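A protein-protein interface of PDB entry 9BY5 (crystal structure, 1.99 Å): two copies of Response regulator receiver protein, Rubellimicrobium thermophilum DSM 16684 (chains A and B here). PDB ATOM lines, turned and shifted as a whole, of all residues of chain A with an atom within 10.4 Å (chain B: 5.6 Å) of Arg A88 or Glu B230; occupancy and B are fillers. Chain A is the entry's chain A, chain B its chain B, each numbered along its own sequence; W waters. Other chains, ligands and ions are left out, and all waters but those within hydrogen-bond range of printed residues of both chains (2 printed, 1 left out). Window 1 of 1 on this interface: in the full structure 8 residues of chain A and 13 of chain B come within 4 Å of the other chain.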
ATOM      1  N   GLY A  85       4.501  10.129 -29.543  1.00  0.00           N
ATOM      2  CA  GLY A  85       5.154   9.248 -28.589  1.00  0.00           C
ATOM      3  C   GLY A  85       4.141   8.399 -27.845  1.00  0.00           C
ATOM      4  O   GLY A  85       3.566   7.469 -28.410  1.00  0.00           O
ATOM      5  N   LEU A  86       3.909   8.732 -26.578  1.00  0.00           N
ATOM      6  CA  LEU A  86       2.919   8.028 -25.770  1.00  0.00           C
ATOM      7  C   LEU A  86       1.512   8.544 -26.075  1.00  0.00           C
ATOM      8  O   LEU A  86       1.273   9.753 -26.110  1.00  0.00           O
ATOM      9  CB  LEU A  86       3.245   8.200 -24.287  1.00  0.00           C
ATOM     10  CG  LEU A  86       2.484   7.411 -23.224  1.00  0.00           C
ATOM     11  CD1 LEU A  86       2.225   5.966 -23.663  1.00  0.00           C
ATOM     12  CD2 LEU A  86       3.247   7.453 -21.916  1.00  0.00           C
ATOM     13  N   ALA A  87       0.557   7.650 -26.266  1.00  0.00           N
ATOM     14  CA  ALA A  87      -0.844   8.031 -26.517  1.00  0.00           C
ATOM     15  C   ALA A  87      -1.346   8.975 -25.430  1.00  0.00           C
ATOM     16  O   ALA A  87      -0.935   8.834 -24.271  1.00  0.00           O
ATOM     17  CB  ALA A  87      -1.688   6.790 -26.571  1.00  0.00           C
ATOM     18  N   ARG A  88      -2.241   9.887 -25.797  1.00  0.00           N
ATOM     19  CA  ARG A  88      -2.798  10.861 -24.832  1.00  0.00           C
ATOM     20  C   ARG A  88      -3.785  10.119 -23.937  1.00  0.00           C
ATOM     21  O   ARG A  88      -4.122  10.667 -22.885  1.00  0.00           O
ATOM     22  CB  ARG A  88      -3.465  12.044 -25.539  1.00  0.00           C
ATOM     23  CG  ARG A  88      -2.570  13.248 -25.792  1.00  0.00           C
ATOM     24  CD  ARG A  88      -1.981  13.809 -24.513  1.00  0.00           C
ATOM     25  NE  ARG A  88      -2.938  14.486 -23.632  1.00  0.00           N
ATOM     26  CZ  ARG A  88      -3.060  14.294 -22.323  1.00  0.00           C
ATOM     27  NH1 ARG A  88      -2.091  13.751 -21.618  1.00  0.00           N
ATOM     28  NH2 ARG A  88      -4.167  14.648 -21.705  1.00  0.00           N
ATOM     29  N   ALA A  89      -4.268   8.961 -24.376  1.00  0.00           N
ATOM     30  CA  ALA A  89      -5.173   8.123 -23.567  1.00  0.00           C
ATOM     31  C   ALA A  89      -4.328   7.488 -22.477  1.00  0.00           C
ATOM     32  O   ALA A  89      -4.794   7.510 -21.358  1.00  0.00           O
ATOM     33  CB  ALA A  89      -5.839   7.087 -24.420  1.00  0.00           C
ATOM     34  N   ALA A  90      -3.194   6.880 -22.822  1.00  0.00           N
ATOM     35  CA  ALA A  90      -2.247   6.353 -21.841  1.00  0.00           C
ATOM     36  C   ALA A  90      -1.820   7.440 -20.858  1.00  0.00           C
ATOM     37  O   ALA A  90      -1.812   7.223 -19.640  1.00  0.00           O
ATOM     38  CB  ALA A  90      -1.027   5.753 -22.545  1.00  0.00           C
ATOM     39  N   GLN A  91      -1.507   8.629 -21.375  1.00  0.00           N
ATOM     40  CA  GLN A  91      -1.023   9.750 -20.535  1.00  0.00           C
ATOM     41  C   GLN A  91      -2.103  10.132 -19.510  1.00  0.00           C
ATOM     42  O   GLN A  91      -1.727  10.491 -18.398  1.00  0.00           O
ATOM     43  CB  GLN A  91      -0.611  10.919 -21.428  1.00  0.00           C
ATOM     44  CG  GLN A  91       0.733  10.723 -22.121  1.00  0.00           C
ATOM     45  CD  GLN A  91       1.077  11.821 -23.105  1.00  0.00           C
ATOM     46  OE1 GLN A  91       0.612  12.954 -23.006  1.00  0.00           O
ATOM     47  NE2 GLN A  91       1.920  11.508 -24.071  1.00  0.00           N
ATOM     48  N   ARG A  92      -3.380  10.078 -19.880  1.00  0.00           N
ATOM     49  CA  ARG A  92      -4.497  10.447 -18.972  1.00  0.00           C
ATOM     50  C   ARG A  92      -4.640   9.345 -17.916  1.00  0.00           C
ATOM     51  O   ARG A  92      -4.778   9.683 -16.749  1.00  0.00           O
ATOM     52  CB  ARG A  92      -5.798  10.665 -19.749  1.00  0.00           C
ATOM     53  CG  ARG A  92      -5.834  12.002 -20.472  1.00  0.00           C
ATOM     54  CD  ARG A  92      -7.161  12.303 -21.136  1.00  0.00           C
ATOM     55  NE  ARG A  92      -8.112  12.888 -20.185  1.00  0.00           N
ATOM     56  CZ  ARG A  92      -9.095  13.732 -20.471  1.00  0.00           C
ATOM     57  NH1 ARG A  92      -8.880  14.812 -21.196  1.00  0.00           N
ATOM     58  NH2 ARG A  92     -10.300  13.511 -19.989  1.00  0.00           N
ATOM     59  N   HIS A  93      -4.560   8.085 -18.324  1.00  0.00           N
ATOM     60  CA  HIS A  93      -4.665   6.943 -17.385  1.00  0.00           C
ATOM     61  C   HIS A  93      -3.498   7.012 -16.397  1.00  0.00           C
ATOM     62  O   HIS A  93      -3.748   6.896 -15.190  1.00  0.00           O
ATOM     63  CB  HIS A  93      -4.713   5.615 -18.140  1.00  0.00           C
ATOM     64  CG  HIS A  93      -5.396   4.513 -17.402  1.00  0.00           C
ATOM     65  ND1 HIS A  93      -5.577   4.475 -16.036  1.00  0.00           N
ATOM     66  CD2 HIS A  93      -5.939   3.388 -17.876  1.00  0.00           C
ATOM     67  CE1 HIS A  93      -6.211   3.360 -15.710  1.00  0.00           C
ATOM     68  NE2 HIS A  93      -6.442   2.685 -16.813  1.00  0.00           N
ATOM     69  N   LEU A  94      -2.267   7.178 -16.881  1.00  0.00           N
ATOM     70  CA  LEU A  94      -1.113   7.188 -15.989  1.00  0.00           C
ATOM     71  C   LEU A  94      -1.147   8.370 -15.024  1.00  0.00           C
ATOM     72  O   LEU A  94      -0.698   8.246 -13.876  1.00  0.00           O
ATOM     73  CB  LEU A  94       0.177   7.212 -16.809  1.00  0.00           C
ATOM     74  CG  LEU A  94       0.504   5.873 -17.486  1.00  0.00           C
ATOM     75  CD1 LEU A  94       1.441   6.043 -18.686  1.00  0.00           C
ATOM     76  CD2 LEU A  94       1.078   4.893 -16.469  1.00  0.00           C
ATOM     77  N   ALA A  95      -1.670   9.521 -15.471  1.00  0.00           N
ATOM     78  CA  ALA A  95      -1.694  10.725 -14.642  1.00  0.00           C
ATOM     79  C   ALA A  95      -2.571  10.578 -13.404  1.00  0.00           C
ATOM     80  O   ALA A  95      -2.397  11.345 -12.454  1.00  0.00           O
ATOM     81  CB  ALA A  95      -2.166  11.933 -15.462  1.00  0.00           C
ATOM     82  N   ARG A  96      -3.517   9.640 -13.402  1.00  0.00           N
ATOM     83  CA  ARG A  96      -4.376   9.395 -12.249  1.00  0.00           C
ATOM     84  C   ARG A  96      -3.792   8.395 -11.256  1.00  0.00           C
ATOM     85  O   ARG A  96      -4.478   8.035 -10.296  1.00  0.00           O
ATOM     86  CB  ARG A  96      -5.750   8.891 -12.708  1.00  0.00           C
ATOM     87  CG  ARG A  96      -6.383   9.713 -13.814  1.00  0.00           C
ATOM     88  CD  ARG A  96      -7.799   9.247 -14.165  1.00  0.00           C
ATOM     89  NE  ARG A  96      -7.871   7.818 -14.457  1.00  0.00           N
ATOM     90  CZ  ARG A  96      -8.439   7.295 -15.539  1.00  0.00           C
ATOM     91  NH1 ARG A  96      -8.960   8.060 -16.486  1.00  0.00           N
ATOM     92  NH2 ARG A  96      -8.484   5.973 -15.675  1.00  0.00           N
ATOM     93  N   LEU A  97      -2.562   7.931 -11.460  1.00  0.00           N
ATOM     94  CA  LEU A  97      -1.961   6.933 -10.583  1.00  0.00           C
ATOM     95  C   LEU A  97      -1.190   7.627  -9.474  1.00  0.00           C
ATOM     96  O   LEU A  97      -0.580   8.676  -9.691  1.00  0.00           O
ATOM     97  CB  LEU A  97      -1.017   6.014 -11.363  1.00  0.00           C
ATOM     98  CG  LEU A  97      -1.674   5.146 -12.439  1.00  0.00           C
ATOM     99  CD1 LEU A  97      -0.672   4.247 -13.162  1.00  0.00           C
ATOM    100  CD2 LEU A  97      -2.772   4.325 -11.822  1.00  0.00           C
ATOM    101  N   PHE A 262      -2.461   0.069 -19.097  1.00  0.00           N
ATOM    102  CA  PHE A 262      -2.401   1.539 -19.102  1.00  0.00           C
ATOM    103  C   PHE A 262      -2.078   2.093 -20.480  1.00  0.00           C
ATOM    104  O   PHE A 262      -2.345   3.270 -20.756  1.00  0.00           O
ATOM    105  CB  PHE A 262      -1.335   2.061 -18.120  1.00  0.00           C
ATOM    106  CG  PHE A 262      -1.571   1.663 -16.681  1.00  0.00           C
ATOM    107  CD1 PHE A 262      -2.809   1.839 -16.088  1.00  0.00           C
ATOM    108  CD2 PHE A 262      -0.543   1.114 -15.921  1.00  0.00           C
ATOM    109  CE1 PHE A 262      -3.025   1.464 -14.767  1.00  0.00           C
ATOM    110  CE2 PHE A 262      -0.747   0.738 -14.599  1.00  0.00           C
ATOM    111  CZ  PHE A 262      -1.988   0.915 -14.020  1.00  0.00           C
ATOM    112  N   PHE A 263      -1.481   1.287 -21.346  1.00  0.00           N
ATOM    113  CA  PHE A 263      -1.075   1.767 -22.653  1.00  0.00           C
ATOM    114  C   PHE A 263      -2.046   1.348 -23.749  1.00  0.00           C
ATOM    115  O   PHE A 263      -1.752   1.552 -24.928  1.00  0.00           O
ATOM    116  CB  PHE A 263       0.359   1.306 -22.941  1.00  0.00           C
ATOM    117  CG  PHE A 263       1.363   1.777 -21.899  1.00  0.00           C
ATOM    118  CD1 PHE A 263       1.995   3.002 -22.033  1.00  0.00           C
ATOM    119  CD2 PHE A 263       1.650   1.012 -20.771  1.00  0.00           C
ATOM    120  CE1 PHE A 263       2.902   3.466 -21.083  1.00  0.00           C
ATOM    121  CE2 PHE A 263       2.559   1.463 -19.806  1.00  0.00           C
ATOM    122  CZ  PHE A 263       3.188   2.703 -19.963  1.00  0.00           C
ATOM    123  N   ALA A 264      -3.183   0.743 -23.376  1.00  0.00           N
ATOM    124  CA  ALA A 264      -4.353   0.488 -24.249  1.00  0.00           C
ATOM    125  C   ALA A 264      -4.025  -0.061 -25.634  1.00  0.00           C
ATOM    126  O   ALA A 264      -4.904  -0.587 -26.346  1.00  0.00           O
ATOM    127  CB  ALA A 264      -5.174   1.776 -24.386  1.00  0.00           C
ATOM    128  N   PRO B  20      -8.384  18.950 -13.832  1.00  0.00           N
ATOM    129  CA  PRO B  20      -7.263  19.534 -14.600  1.00  0.00           C
ATOM    130  C   PRO B  20      -7.680  19.958 -16.004  1.00  0.00           C
ATOM    131  O   PRO B  20      -7.198  20.999 -16.470  1.00  0.00           O
ATOM    132  CB  PRO B  20      -6.242  18.413 -14.653  1.00  0.00           C
ATOM    133  CG  PRO B  20      -6.539  17.609 -13.415  1.00  0.00           C
ATOM    134  CD  PRO B  20      -8.014  17.582 -13.363  1.00  0.00           C
ATOM    135  N   TYR B  21      -8.528  19.181 -16.659  1.00  0.00           N
ATOM    136  CA  TYR B  21      -8.952  19.467 -18.054  1.00  0.00           C
ATOM    137  C   TYR B  21      -9.958  20.579 -18.057  1.00  0.00           C
ATOM    138  O   TYR B  21      -9.985  21.303 -19.034  1.00  0.00           O
ATOM    139  CB  TYR B  21      -9.512  18.187 -18.659  1.00  0.00           C
ATOM    140  CG  TYR B  21      -8.560  17.029 -18.456  1.00  0.00           C
ATOM    141  CD1 TYR B  21      -7.289  17.053 -19.009  1.00  0.00           C
ATOM    142  CD2 TYR B  21      -8.910  15.964 -17.644  1.00  0.00           C
ATOM    143  CE1 TYR B  21      -6.400  16.020 -18.791  1.00  0.00           C
ATOM    144  CE2 TYR B  21      -8.032  14.925 -17.417  1.00  0.00           C
ATOM    145  CZ  TYR B  21      -6.779  14.960 -17.993  1.00  0.00           C
ATOM    146  OH  TYR B  21      -5.907  13.954 -17.780  1.00  0.00           O
ATOM    147  N   ARG B  24      -7.880  23.563 -18.102  1.00  0.00           N
ATOM    148  CA  ARG B  24      -7.319  23.836 -19.425  1.00  0.00           C
ATOM    149  C   ARG B  24      -8.309  24.612 -20.279  1.00  0.00           C
ATOM    150  O   ARG B  24      -7.969  25.636 -20.887  1.00  0.00           O
ATOM    151  CB  ARG B  24      -6.921  22.525 -20.115  1.00  0.00           C
ATOM    152  CG  ARG B  24      -6.261  22.717 -21.477  1.00  0.00           C
ATOM    153  CD  ARG B  24      -5.912  21.381 -22.102  1.00  0.00           C
ATOM    154  NE  ARG B  24      -6.988  20.399 -21.978  1.00  0.00           N
ATOM    155  CZ  ARG B  24      -6.826  19.110 -22.228  1.00  0.00           C
ATOM    156  NH1 ARG B  24      -5.617  18.592 -22.407  1.00  0.00           N
ATOM    157  NH2 ARG B  24      -7.894  18.313 -22.273  1.00  0.00           N
ATOM    158  N   ALA B 227       3.960  16.763 -23.541  1.00  0.00           N
ATOM    159  CA  ALA B 227       3.317  15.566 -23.018  1.00  0.00           C
ATOM    160  C   ALA B 227       2.976  15.791 -21.545  1.00  0.00           C
ATOM    161  O   ALA B 227       3.531  16.672 -20.889  1.00  0.00           O
ATOM    162  CB  ALA B 227       4.217  14.338 -23.192  1.00  0.00           C
ATOM    163  N   PHE B 228       2.025  15.021 -21.034  1.00  0.00           N
ATOM    164  CA  PHE B 228       1.570  15.155 -19.655  1.00  0.00           C
ATOM    165  C   PHE B 228       1.250  16.612 -19.283  1.00  0.00           C
ATOM    166  O   PHE B 228       1.766  17.138 -18.301  1.00  0.00           O
ATOM    167  CB  PHE B 228       2.588  14.563 -18.691  1.00  0.00           C
ATOM    168  CG  PHE B 228       2.637  13.055 -18.756  1.00  0.00           C
ATOM    169  CD1 PHE B 228       1.609  12.291 -18.222  1.00  0.00           C
ATOM    170  CD2 PHE B 228       3.681  12.407 -19.386  1.00  0.00           C
ATOM    171  CE1 PHE B 228       1.629  10.899 -18.320  1.00  0.00           C
ATOM    172  CE2 PHE B 228       3.708  11.020 -19.481  1.00  0.00           C
ATOM    173  CZ  PHE B 228       2.686  10.271 -18.948  1.00  0.00           C
ATOM    174  N   PRO B 229       0.354  17.260 -20.027  1.00  0.00           N
ATOM    175  CA  PRO B 229      -0.056  18.615 -19.638  1.00  0.00           C
ATOM    176  C   PRO B 229      -0.650  18.656 -18.237  1.00  0.00           C
ATOM    177  O   PRO B 229      -0.688  19.727 -17.632  1.00  0.00           O
ATOM    178  CB  PRO B 229      -1.105  18.983 -20.705  1.00  0.00           C
ATOM    179  CG  PRO B 229      -1.664  17.613 -21.145  1.00  0.00           C
ATOM    180  CD  PRO B 229      -0.432  16.742 -21.172  1.00  0.00           C
ATOM    181  N   GLU B 230      -1.096  17.516 -17.716  1.00  0.00           N
ATOM    182  CA  GLU B 230      -1.697  17.421 -16.363  1.00  0.00           C
ATOM    183  C   GLU B 230      -0.732  18.002 -15.313  1.00  0.00           C
ATOM    184  O   GLU B 230      -1.228  18.523 -14.315  1.00  0.00           O
ATOM    185  CB  GLU B 230      -2.052  15.969 -16.063  1.00  0.00           C
ATOM    186  CG  GLU B 230      -3.137  15.403 -16.973  1.00  0.00           C
ATOM    187  CD  GLU B 230      -2.620  14.604 -18.154  1.00  0.00           C
ATOM    188  OE1 GLU B 230      -1.503  14.859 -18.620  1.00  0.00           O
ATOM    189  OE2 GLU B 230      -3.345  13.714 -18.609  1.00  0.00           O
ATOM    190  N   ARG B 231       0.581  17.928 -15.532  1.00  0.00           N
ATOM    191  CA  ARG B 231       1.544  18.455 -14.576  1.00  0.00           C
ATOM    192  C   ARG B 231       1.583  19.974 -14.548  1.00  0.00           C
ATOM    193  O   ARG B 231       2.154  20.535 -13.611  1.00  0.00           O
ATOM    194  CB  ARG B 231       2.936  17.876 -14.876  1.00  0.00           C
ATOM    195  CG  ARG B 231       3.580  18.404 -16.144  1.00  0.00           C
ATOM    196  CD  ARG B 231       4.677  17.463 -16.676  1.00  0.00           C
ATOM    197  NE  ARG B 231       5.806  18.203 -17.233  1.00  0.00           N
ATOM    198  CZ  ARG B 231       6.962  17.661 -17.600  1.00  0.00           C
ATOM    199  NH1 ARG B 231       7.175  16.357 -17.515  1.00  0.00           N
ATOM    200  NH2 ARG B 231       7.928  18.447 -18.073  1.00  0.00           N
ATOM    201  N   LEU B 232       0.988  20.648 -15.535  1.00  0.00           N
ATOM    202  CA  LEU B 232       0.857  22.100 -15.559  1.00  0.00           C
ATOM    203  C   LEU B 232      -0.582  22.566 -15.347  1.00  0.00           C
ATOM    204  O   LEU B 232      -0.878  23.742 -15.577  1.00  0.00           O
ATOM    205  CB  LEU B 232       1.387  22.654 -16.888  1.00  0.00           C
ATOM    206  CG  LEU B 232       2.888  22.464 -17.080  1.00  0.00           C
ATOM    207  CD1 LEU B 232       3.286  22.840 -18.492  1.00  0.00           C
ATOM    208  CD2 LEU B 232       3.655  23.307 -16.044  1.00  0.00           C
ATOM    209  N   LEU B 233      -1.473  21.679 -14.923  1.00  0.00           N
ATOM    210  CA  LEU B 233      -2.894  21.968 -14.755  1.00  0.00           C
ATOM    211  C   LEU B 233      -3.352  21.702 -13.323  1.00  0.00           C
ATOM    212  O   LEU B 233      -4.490  21.276 -13.093  1.00  0.00           O
ATOM    213  CB  LEU B 233      -3.725  21.129 -15.726  1.00  0.00           C
ATOM    214  CG  LEU B 233      -3.560  21.492 -17.213  1.00  0.00           C
ATOM    215  CD1 LEU B 233      -4.197  20.425 -18.093  1.00  0.00           C
ATOM    216  CD2 LEU B 233      -4.117  22.899 -17.526  1.00  0.00           C
ATOM    217  N   THR B 234      -2.459  21.896 -12.352  1.00  0.00           N
ATOM    218  CA  THR B 234      -2.792  21.646 -10.952  1.00  0.00           C
ATOM    219  C   THR B 234      -3.379  22.863 -10.243  1.00  0.00           C
ATOM    220  O   THR B 234      -4.012  22.705  -9.195  1.00  0.00           O
ATOM    221  CB  THR B 234      -1.547  21.193 -10.182  1.00  0.00           C
ATOM    222  OG1 THR B 234      -0.686  22.326  -9.982  1.00  0.00           O
ATOM    223  CG2 THR B 234      -0.804  20.121 -10.932  1.00  0.00           C
ATOM    224  N   GLU B 239       1.268  28.716 -13.765  1.00  0.00           N
ATOM    225  CA  GLU B 239       1.132  27.748 -14.845  1.00  0.00           C
ATOM    226  C   GLU B 239       0.607  28.464 -16.082  1.00  0.00           C
ATOM    227  O   GLU B 239      -0.006  29.532 -15.971  1.00  0.00           O
ATOM    228  CB  GLU B 239       0.200  26.590 -14.453  1.00  0.00           C
ATOM    229  CG  GLU B 239       0.778  25.637 -13.385  1.00  0.00           C
ATOM    230  CD  GLU B 239      -0.272  24.704 -12.783  1.00  0.00           C
ATOM    231  OE1 GLU B 239      -1.405  25.170 -12.530  1.00  0.00           O
ATOM    232  OE2 GLU B 239       0.045  23.514 -12.499  1.00  0.00           O
ATOM    233  N   SER B 245      -1.240  19.418 -26.124  1.00  0.00           N
ATOM    234  CA  SER B 245      -0.649  18.141 -25.683  1.00  0.00           C
ATOM    235  C   SER B 245       0.263  17.575 -26.768  1.00  0.00           C
ATOM    236  O   SER B 245       0.176  18.059 -27.882  1.00  0.00           O
ATOM    237  CB  SER B 245      -1.716  17.166 -25.317  1.00  0.00           C
ATOM    238  OG  SER B 245      -2.745  17.803 -24.575  1.00  0.00           O
ATOM    239  N   LYS B 246       1.173  16.679 -26.416  1.00  0.00           N
ATOM    240  CA  LYS B 246       2.010  15.948 -27.389  1.00  0.00           C
ATOM    241  C   LYS B 246       1.732  14.492 -27.024  1.00  0.00           C
ATOM    242  O   LYS B 246       1.874  14.220 -25.833  1.00  0.00           O
ATOM    243  CB  LYS B 246       3.503  16.257 -27.293  1.00  0.00           C
ATOM    244  CG  LYS B 246       3.887  17.662 -27.656  1.00  0.00           C
ATOM    245  CD  LYS B 246       5.316  17.804 -28.156  1.00  0.00           C
ATOM    246  CE  LYS B 246       6.070  18.835 -27.398  1.00  0.00           C
ATOM    247  NZ  LYS B 246       7.490  18.769 -27.736  1.00  0.00           N
ATOM    248  N   PRO B 247       1.224  13.603 -27.905  1.00  0.00           N
ATOM    249  CA  PRO B 247       0.928  13.916 -29.315  1.00  0.00           C
ATOM    250  C   PRO B 247      -0.293  14.810 -29.436  1.00  0.00           C
ATOM    251  O   PRO B 247      -1.179  14.812 -28.586  1.00  0.00           O
ATOM    252  CB  PRO B 247       0.675  12.530 -29.934  1.00  0.00           C
ATOM    253  CG  PRO B 247       0.063  11.750 -28.791  1.00  0.00           C
ATOM    254  CD  PRO B 247       0.832  12.221 -27.562  1.00  0.00           C
HETATM  255  O   HOH W   1      -5.027  16.075 -25.252  1.00  0.00           O
HETATM  256  O   HOH W   2      -6.167  12.035 -16.065  1.00  0.00           O
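OH of Tyr B21 lies close to NE of Arg A92, at 3.4 Å.
NE2 of Gln A91 is in hydrogen-bond range of O of Lys B246 (3.2 Å).
The guanidinium group (NE) of Arg A88 lies close to the side-chain hydroxyl (OG) of Ser B245 (3.5 Å).
The side-chain amide oxygen (OE1) of Gln A91 is in hydrogen-bond range of the backbone NH (N) of Phe B228, 3.2 Å away.
OE1 of Glu B230 is in salt-bridge range of NH1 of Arg A88 (3.2 Å).
No position is printed for both chains.
Of the 15 pairs that touch across the chains among the printed residues, none has its exchanged pair printed and touching as well.
Water W2 lies within hydrogen-bond range of OH of Tyr B21 (2.6 Å) and O of Arg A92 (2.8 Å).
Water W1 lies within hydrogen-bond range of the side-chain hydroxyl (OG) of Ser B245 (2.9 Å) and the guanidinium group (NE) of Arg A88 (3.1 Å).
Among the printed residues, pairs that only touch across the chains: Leu A86 with Pro B247 (2.9 Å), Arg A88 with Pro B229 (3.4 Å), Arg A92 with Glu B230 (3.5 Å), Arg A88 with Pro B247 (3.5 Å), Gln A91 with Glu B230 (3.6 Å), Gln A91 with Pro B247 (3.7 Å), Gln A91 with Ala B227 (3.7 Å), Arg A92 with Arg B24 (3.8 Å), Ala A95 with Glu B230 (3.8 Å) and Arg A88 with Tyr B21 (3.9 Å).
Hydrophobic or aromatic side chains of chain B within 4 Å of the printed part of chain A: Tyr B21, Ala B227, Phe B228, Pro B229 and Pro B247.
Hydrophobic or aromatic side chains of chain A within 4 Å of the printed part of chain B: Ala A95.
Among the printed residues, Asp or Glu carboxylates within 4 Å of a Lys or Arg side-chain nitrogen of the other chain: Arg A88 with Glu B230 (3.2 Å).
The side-chain amide nitrogen (NE2) of Gln A91 is in hydrogen-bond range of the backbone carbonyl oxygen (O) of Leu A86 (2.8 Å).
The side-chain carboxylate (OE2) of Glu B230 is in hydrogen-bond range of the side-chain hydroxyl (OH) of Tyr B21.
The side-chain amide oxygen (OE1) of Gln A91 sits close to the guanidinium group (NH1) of Arg A88 (3.1 Å).
Arg A88 touches just these residues of chain B: Tyr B21, Pro B229, Glu B230, Ser B245 and Pro B247.
Glu B230 touches just these residues of chain A: Arg A88 (3.2 Å), Gln A91 (3.6 Å), Arg A92 (3.5 Å) and Ala A95 (3.8 Å).
Pro B229 touches just one residue of chain A: Arg A88 (3.4 Å).
No residue of chain A comes within 4 Å of Leu B233.
Printed residues of chain A within 4 Å of Tyr B21: Arg A88 and Arg A92.
Of the printed residues of chain B, Leu A86 touches Pro B247 (2.9 Å).
Printed residues of chain B within 4 Å of Ala A95: Glu B230 (3.8 Å).
Arg B231 touches none of the printed residues of chain A.
Gly A85 touches none of the printed residues of chain B.
The nearest residue of chain A that does not touch Glu B230 is His A93 (5.8 Å).
The nearest printed residue of chain A that does not touch Arg B24 is Arg A88 (4.3 Å).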
